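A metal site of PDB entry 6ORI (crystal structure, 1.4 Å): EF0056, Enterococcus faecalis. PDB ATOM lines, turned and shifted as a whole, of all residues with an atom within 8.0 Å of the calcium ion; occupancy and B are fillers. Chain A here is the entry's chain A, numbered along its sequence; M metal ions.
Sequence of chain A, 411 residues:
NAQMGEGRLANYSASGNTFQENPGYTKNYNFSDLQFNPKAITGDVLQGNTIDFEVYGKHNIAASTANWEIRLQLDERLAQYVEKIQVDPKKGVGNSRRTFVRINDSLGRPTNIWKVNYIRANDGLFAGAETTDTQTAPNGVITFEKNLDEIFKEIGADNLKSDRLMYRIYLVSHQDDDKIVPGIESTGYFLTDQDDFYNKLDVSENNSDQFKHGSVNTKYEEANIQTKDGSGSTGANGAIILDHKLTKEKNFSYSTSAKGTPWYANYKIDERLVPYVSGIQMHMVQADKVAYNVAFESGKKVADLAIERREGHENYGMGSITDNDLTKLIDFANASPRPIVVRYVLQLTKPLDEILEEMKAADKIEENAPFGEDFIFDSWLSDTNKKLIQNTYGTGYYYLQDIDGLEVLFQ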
ATOM      1  N   ARG A  77     -14.089  19.442 -14.572  1.00  0.00           N
ATOM      2  CA  ARG A  77     -15.458  19.840 -14.272  1.00  0.00           C
ATOM      3  C   ARG A  77     -15.500  21.073 -13.388  1.00  0.00           C
ATOM      4  O   ARG A  77     -16.466  21.831 -13.413  1.00  0.00           O
ATOM      5  CB  ARG A  77     -16.206  18.667 -13.623  1.00  0.00           C
ATOM      6  CG  ARG A  77     -16.429  17.514 -14.595  1.00  0.00           C
ATOM      7  CD  ARG A  77     -16.915  16.244 -13.892  1.00  0.00           C
ATOM      8  NE  ARG A  77     -15.906  15.732 -12.983  1.00  0.00           N
ATOM      9  CZ  ARG A  77     -16.128  14.858 -12.011  1.00  0.00           C
ATOM     10  NH1 ARG A  77     -17.339  14.349 -11.807  1.00  0.00           N
ATOM     11  NH2 ARG A  77     -15.136  14.477 -11.226  1.00  0.00           N
ATOM     12  N   ASN A 159     -23.091  12.259 -11.166  1.00  0.00           N
ATOM     13  CA  ASN A 159     -21.730  12.255 -11.693  1.00  0.00           C
ATOM     14  C   ASN A 159     -20.698  12.574 -10.614  1.00  0.00           C
ATOM     15  O   ASN A 159     -19.581  12.078 -10.659  1.00  0.00           O
ATOM     16  CB  ASN A 159     -21.623  13.205 -12.878  1.00  0.00           C
ATOM     17  CG  ASN A 159     -22.459  12.745 -14.046  1.00  0.00           C
ATOM     18  OD1 ASN A 159     -22.363  11.593 -14.460  1.00  0.00           O
ATOM     19  ND2 ASN A 159     -23.321  13.623 -14.557  1.00  0.00           N
ATOM     20  N   LYS A 161     -21.046  11.593  -7.620  1.00  0.00           N
ATOM     21  CA  LYS A 161     -20.978  10.361  -6.868  1.00  0.00           C
ATOM     22  C   LYS A 161     -20.029   9.370  -7.550  1.00  0.00           C
ATOM     23  O   LYS A 161     -19.237   8.708  -6.895  1.00  0.00           O
ATOM     24  CB  LYS A 161     -22.378   9.768  -6.728  1.00  0.00           C
ATOM     25  CG  LYS A 161     -22.528   8.600  -5.774  1.00  0.00           C
ATOM     26  CD  LYS A 161     -23.832   8.718  -4.971  1.00  0.00           C
ATOM     27  CE  LYS A 161     -25.078   8.920  -5.860  1.00  0.00           C
ATOM     28  NZ  LYS A 161     -26.181   9.642  -5.143  1.00  0.00           N
ATOM     29  N   SER A 162     -20.104   9.293  -8.867  1.00  0.00           N
ATOM     30  CA  SER A 162     -19.375   8.257  -9.582  1.00  0.00           C
ATOM     31  C   SER A 162     -17.928   8.627  -9.948  1.00  0.00           C
ATOM     32  O   SER A 162     -17.097   7.759 -10.104  1.00  0.00           O
ATOM     33  CB  SER A 162     -20.143   7.826 -10.836  1.00  0.00           C
ATOM     34  OG  SER A 162     -20.223   8.878 -11.776  1.00  0.00           O
ATOM     35  N   ASP A 163     -17.660   9.913 -10.180  1.00  0.00           N
ATOM     36  CA  ASP A 163     -16.302  10.413 -10.440  1.00  0.00           C
ATOM     37  C   ASP A 163     -15.997  11.502  -9.406  1.00  0.00           C
ATOM     38  O   ASP A 163     -16.592  12.596  -9.428  1.00  0.00           O
ATOM     39  CB  ASP A 163     -16.181  11.032 -11.845  1.00  0.00           C
ATOM     40  CG  ASP A 163     -15.993  10.028 -12.970  1.00  0.00           C
ATOM     41  OD1 ASP A 163     -15.728   8.847 -12.717  1.00  0.00           O
ATOM     42  OD2 ASP A 163     -16.060  10.450 -14.142  1.00  0.00           O
ATOM     43  N   ARG A 164     -15.083  11.243  -8.493  1.00  0.00           N
ATOM     44  CA  ARG A 164     -14.705  12.264  -7.520  1.00  0.00           C
ATOM     45  C   ARG A 164     -13.964  13.418  -8.215  1.00  0.00           C
ATOM     46  O   ARG A 164     -13.347  13.236  -9.242  1.00  0.00           O
ATOM     47  CB  ARG A 164     -13.832  11.657  -6.420  1.00  0.00           C
ATOM     48  CG  ARG A 164     -14.469  10.464  -5.680  1.00  0.00           C
ATOM     49  CD  ARG A 164     -15.833  10.813  -5.118  1.00  0.00           C
ATOM     50  NE  ARG A 164     -15.837  12.030  -4.302  1.00  0.00           N
ATOM     51  CZ  ARG A 164     -16.067  12.093  -2.992  1.00  0.00           C
ATOM     52  NH1 ARG A 164     -16.051  13.285  -2.393  1.00  0.00           N
ATOM     53  NH2 ARG A 164     -16.309  10.996  -2.271  1.00  0.00           N
ATOM     54  N   ARG A 272     -15.833  -2.671  -2.152  1.00  0.00           N
ATOM     55  CA  ARG A 272     -15.926  -3.472  -3.368  1.00  0.00           C
ATOM     56  C   ARG A 272     -14.640  -4.237  -3.688  1.00  0.00           C
ATOM     57  O   ARG A 272     -14.664  -5.288  -4.347  1.00  0.00           O
ATOM     58  CB  ARG A 272     -16.320  -2.579  -4.532  1.00  0.00           C
ATOM     59  CG  ARG A 272     -17.719  -2.027  -4.438  1.00  0.00           C
ATOM     60  CD  ARG A 272     -17.941  -0.955  -5.476  1.00  0.00           C
ATOM     61  NE  ARG A 272     -17.138   0.212  -5.175  1.00  0.00           N
ATOM     62  CZ  ARG A 272     -16.748   1.109  -6.081  1.00  0.00           C
ATOM     63  NH1 ARG A 272     -17.069   0.983  -7.362  1.00  0.00           N
ATOM     64  NH2 ARG A 272     -16.030   2.139  -5.678  1.00  0.00           N
ATOM     65  N   LYS A 360     -18.792  -5.187 -13.450  1.00  0.00           N
ATOM     66  CA  LYS A 360     -19.796  -4.839 -14.458  1.00  0.00           C
ATOM     67  C   LYS A 360     -20.633  -6.060 -14.836  1.00  0.00           C
ATOM     68  O   LYS A 360     -21.395  -6.596 -14.017  1.00  0.00           O
ATOM     69  CB  LYS A 360     -19.103  -4.294 -15.707  1.00  0.00           C
ATOM     70  CG  LYS A 360     -18.336  -3.007 -15.478  1.00  0.00           C
ATOM     71  CD  LYS A 360     -19.152  -1.763 -15.838  1.00  0.00           C
ATOM     72  CE  LYS A 360     -18.992  -0.637 -14.813  1.00  0.00           C
ATOM     73  NZ  LYS A 360     -17.583  -0.409 -14.380  1.00  0.00           N
ATOM     74  N   GLY A 372     -18.788   1.799 -11.486  1.00  0.00           N
ATOM     75  CA  GLY A 372     -18.359   3.099 -12.006  1.00  0.00           C
ATOM     76  C   GLY A 372     -17.750   3.970 -10.900  1.00  0.00           C
ATOM     77  O   GLY A 372     -16.772   4.701 -11.137  1.00  0.00           O
ATOM     78  N   GLU A 373     -18.338   3.916  -9.718  1.00  0.00           N
ATOM     79  CA  GLU A 373     -17.884   4.738  -8.595  1.00  0.00           C
ATOM     80  C   GLU A 373     -16.396   4.522  -8.365  1.00  0.00           C
ATOM     81  O   GLU A 373     -15.945   3.372  -8.306  1.00  0.00           O
ATOM     82  CB  GLU A 373     -18.687   4.418  -7.333  1.00  0.00           C
ATOM     83  N   ASP A 374     -15.639   5.598  -8.221  1.00  0.00           N
ATOM     84  CA  ASP A 374     -14.187   5.482  -8.059  1.00  0.00           C
ATOM     85  C   ASP A 374     -13.918   4.769  -6.749  1.00  0.00           C
ATOM     86  O   ASP A 374     -14.715   4.831  -5.820  1.00  0.00           O
ATOM     87  CB  ASP A 374     -13.511   6.855  -8.043  1.00  0.00           C
ATOM     88  CG  ASP A 374     -13.694   7.595  -9.345  1.00  0.00           C
ATOM     89  OD1 ASP A 374     -14.057   6.969 -10.380  1.00  0.00           O
ATOM     90  OD2 ASP A 374     -13.482   8.833  -9.327  1.00  0.00           O
ATOM     91  N   PHE A 375     -12.773   4.099  -6.643  1.00  0.00           N
ATOM     92  CA  PHE A 375     -12.440   3.398  -5.407  1.00  0.00           C
ATOM     93  C   PHE A 375     -11.839   4.362  -4.397  1.00  0.00           C
ATOM     94  O   PHE A 375     -10.995   5.179  -4.754  1.00  0.00           O
ATOM     95  CB  PHE A 375     -11.435   2.294  -5.666  1.00  0.00           C
ATOM     96  CG  PHE A 375     -11.924   1.204  -6.557  1.00  0.00           C
ATOM     97  CD1 PHE A 375     -13.033   0.438  -6.223  1.00  0.00           C
ATOM     98  CD2 PHE A 375     -11.245   0.927  -7.727  1.00  0.00           C
ATOM     99  CE1 PHE A 375     -13.449  -0.585  -7.066  1.00  0.00           C
ATOM    100  CE2 PHE A 375     -11.674  -0.085  -8.567  1.00  0.00           C
ATOM    101  CZ  PHE A 375     -12.774  -0.840  -8.230  1.00  0.00           C
ATOM    102  N   TYR A 397      -8.087   8.197  -3.817  1.00  0.00           N
ATOM    103  CA  TYR A 397      -8.987   7.500  -4.707  1.00  0.00           C
ATOM    104  C   TYR A 397      -8.196   6.821  -5.812  1.00  0.00           C
ATOM    105  O   TYR A 397      -7.022   7.147  -6.077  1.00  0.00           O
ATOM    106  CB  TYR A 397     -10.056   8.460  -5.285  1.00  0.00           C
ATOM    107  CG  TYR A 397      -9.588   9.295  -6.426  1.00  0.00           C
ATOM    108  CD1 TYR A 397      -8.708  10.364  -6.234  1.00  0.00           C
ATOM    109  CD2 TYR A 397      -9.989   8.999  -7.713  1.00  0.00           C
ATOM    110  CE1 TYR A 397      -8.272  11.116  -7.291  1.00  0.00           C
ATOM    111  CE2 TYR A 397      -9.539   9.749  -8.773  1.00  0.00           C
ATOM    112  CZ  TYR A 397      -8.675  10.805  -8.552  1.00  0.00           C
ATOM    113  OH  TYR A 397      -8.230  11.533  -9.622  1.00  0.00           O
ATOM    114  N   TYR A 398      -8.850   5.855  -6.440  1.00  0.00           N
ATOM    115  CA  TYR A 398      -8.358   5.260  -7.676  1.00  0.00           C
ATOM    116  C   TYR A 398      -9.504   5.340  -8.690  1.00  0.00           C
ATOM    117  O   TYR A 398     -10.609   4.865  -8.433  1.00  0.00           O
ATOM    118  CB  TYR A 398      -7.892   3.818  -7.493  1.00  0.00           C
ATOM    119  CG  TYR A 398      -7.078   3.370  -8.662  1.00  0.00           C
ATOM    120  CD1 TYR A 398      -7.672   2.782  -9.780  1.00  0.00           C
ATOM    121  CD2 TYR A 398      -5.726   3.572  -8.678  1.00  0.00           C
ATOM    122  CE1 TYR A 398      -6.908   2.415 -10.867  1.00  0.00           C
ATOM    123  CE2 TYR A 398      -4.964   3.189  -9.740  1.00  0.00           C
ATOM    124  CZ  TYR A 398      -5.555   2.628 -10.826  1.00  0.00           C
ATOM    125  OH  TYR A 398      -4.764   2.272 -11.901  1.00  0.00           O
ATOM    126  N   TYR A 399      -9.235   5.983  -9.828  1.00  0.00           N
ATOM    127  CA  TYR A 399     -10.249   6.292 -10.832  1.00  0.00           C
ATOM    128  C   TYR A 399     -10.787   5.062 -11.519  1.00  0.00           C
ATOM    129  O   TYR A 399     -10.036   4.158 -11.876  1.00  0.00           O
ATOM    130  CB  TYR A 399      -9.653   7.195 -11.903  1.00  0.00           C
ATOM    131  CG  TYR A 399     -10.551   7.445 -13.110  1.00  0.00           C
ATOM    132  CD1 TYR A 399     -11.723   8.184 -12.989  1.00  0.00           C
ATOM    133  CD2 TYR A 399     -10.191   6.976 -14.368  1.00  0.00           C
ATOM    134  CE1 TYR A 399     -12.538   8.418 -14.098  1.00  0.00           C
ATOM    135  CE2 TYR A 399     -10.992   7.209 -15.480  1.00  0.00           C
ATOM    136  CZ  TYR A 399     -12.162   7.930 -15.342  1.00  0.00           C
ATOM    137  OH  TYR A 399     -12.949   8.162 -16.458  1.00  0.00           O
ATOM    138  N   LEU A 400     -12.114   5.042 -11.708  1.00  0.00           N
ATOM    139  CA  LEU A 400     -12.822   4.009 -12.480  1.00  0.00           C
ATOM    140  C   LEU A 400     -13.704   4.679 -13.529  1.00  0.00           C
ATOM    141  O   LEU A 400     -14.552   5.502 -13.196  1.00  0.00           O
ATOM    142  CB  LEU A 400     -13.698   3.162 -11.570  1.00  0.00           C
ATOM    143  CG  LEU A 400     -13.522   1.663 -11.704  1.00  0.00           C
ATOM    144  CD1 LEU A 400     -12.057   1.253 -11.476  1.00  0.00           C
ATOM    145  CD2 LEU A 400     -14.458   0.967 -10.722  1.00  0.00           C
ATOM    146  N   GLN A 401     -13.517   4.321 -14.795  1.00  0.00           N
ATOM    147  CA  GLN A 401     -14.272   4.964 -15.884  1.00  0.00           C
ATOM    148  C   GLN A 401     -15.755   4.630 -15.805  1.00  0.00           C
ATOM    149  O   GLN A 401     -16.127   3.466 -15.708  1.00  0.00           O
ATOM    150  CB  GLN A 401     -13.707   4.534 -17.246  1.00  0.00           C
ATOM    151  CG  GLN A 401     -12.280   5.013 -17.484  1.00  0.00           C
ATOM    152  CD  GLN A 401     -11.682   4.503 -18.774  1.00  0.00           C
ATOM    153  OE1 GLN A 401     -12.396   4.150 -19.721  1.00  0.00           O
ATOM    154  NE2 GLN A 401     -10.355   4.443 -18.825  1.00  0.00           N
ATOM    155  N   ASP A 402     -16.590   5.664 -15.844  1.00  0.00           N
ATOM    156  CA  ASP A 402     -18.042   5.489 -15.773  1.00  0.00           C
ATOM    157  C   ASP A 402     -18.583   4.949 -17.095  1.00  0.00           C
ATOM    158  O   ASP A 402     -18.038   5.263 -18.162  1.00  0.00           O
ATOM    159  CB  ASP A 402     -18.722   6.813 -15.439  1.00  0.00           C
ATOM    160  CG  ASP A 402     -18.336   7.363 -14.067  1.00  0.00           C
ATOM    161  OD1 ASP A 402     -17.676   6.621 -13.292  1.00  0.00           O
ATOM    162  OD2 ASP A 402     -18.696   8.520 -13.758  1.00  0.00           O
HETATM  163 CA    CA M   1     -15.858   6.734 -11.835  1.00  0.00          CA
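The guanidinium group (NH2) of Arg 77 sits at hydrogen-bond distance from the backbone carbonyl oxygen (O) of Asp 163 (3.0 Å). The backbone carbonyl oxygen of Asp 374 sits at hydrogen-bond distance from the guanidinium group of Arg 272 (3.0 Å). O of Asn 159 lies within hydrogen-bond range of OG of Ser 162, at 3.4 Å. The backbone NH of Arg 164 lies within hydrogen-bond range of the side-chain carboxylate of Asp 374 (3.0 Å).
Within 4 Å of the calcium ion: Ser 162, Asp 163, Gly 372, Asp 374, Leu 400 and Asp 402. The nearest printed residue that does not touch the calcium ion is Glu 373 (4.2 Å).
O of Leu 400 binds the calcium ion (2.3 Å). The calcium ion is bound by the side-chain carboxylate (OD1) of Asp 163, at 2.3 Å. The calcium ion is bound by the side-chain carboxylate (OD1) of Asp 374 (2.3 Å). The calcium ion is bound by the side-chain carboxylate (OD1) of Asp 402 (2.3 Å). O of Gly 372 is bound to the calcium ion (2.3 Å). The calcium ion is bound by O of Ser 162 (2.4 Å). The calcium ion has six donor atoms within binding distance.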
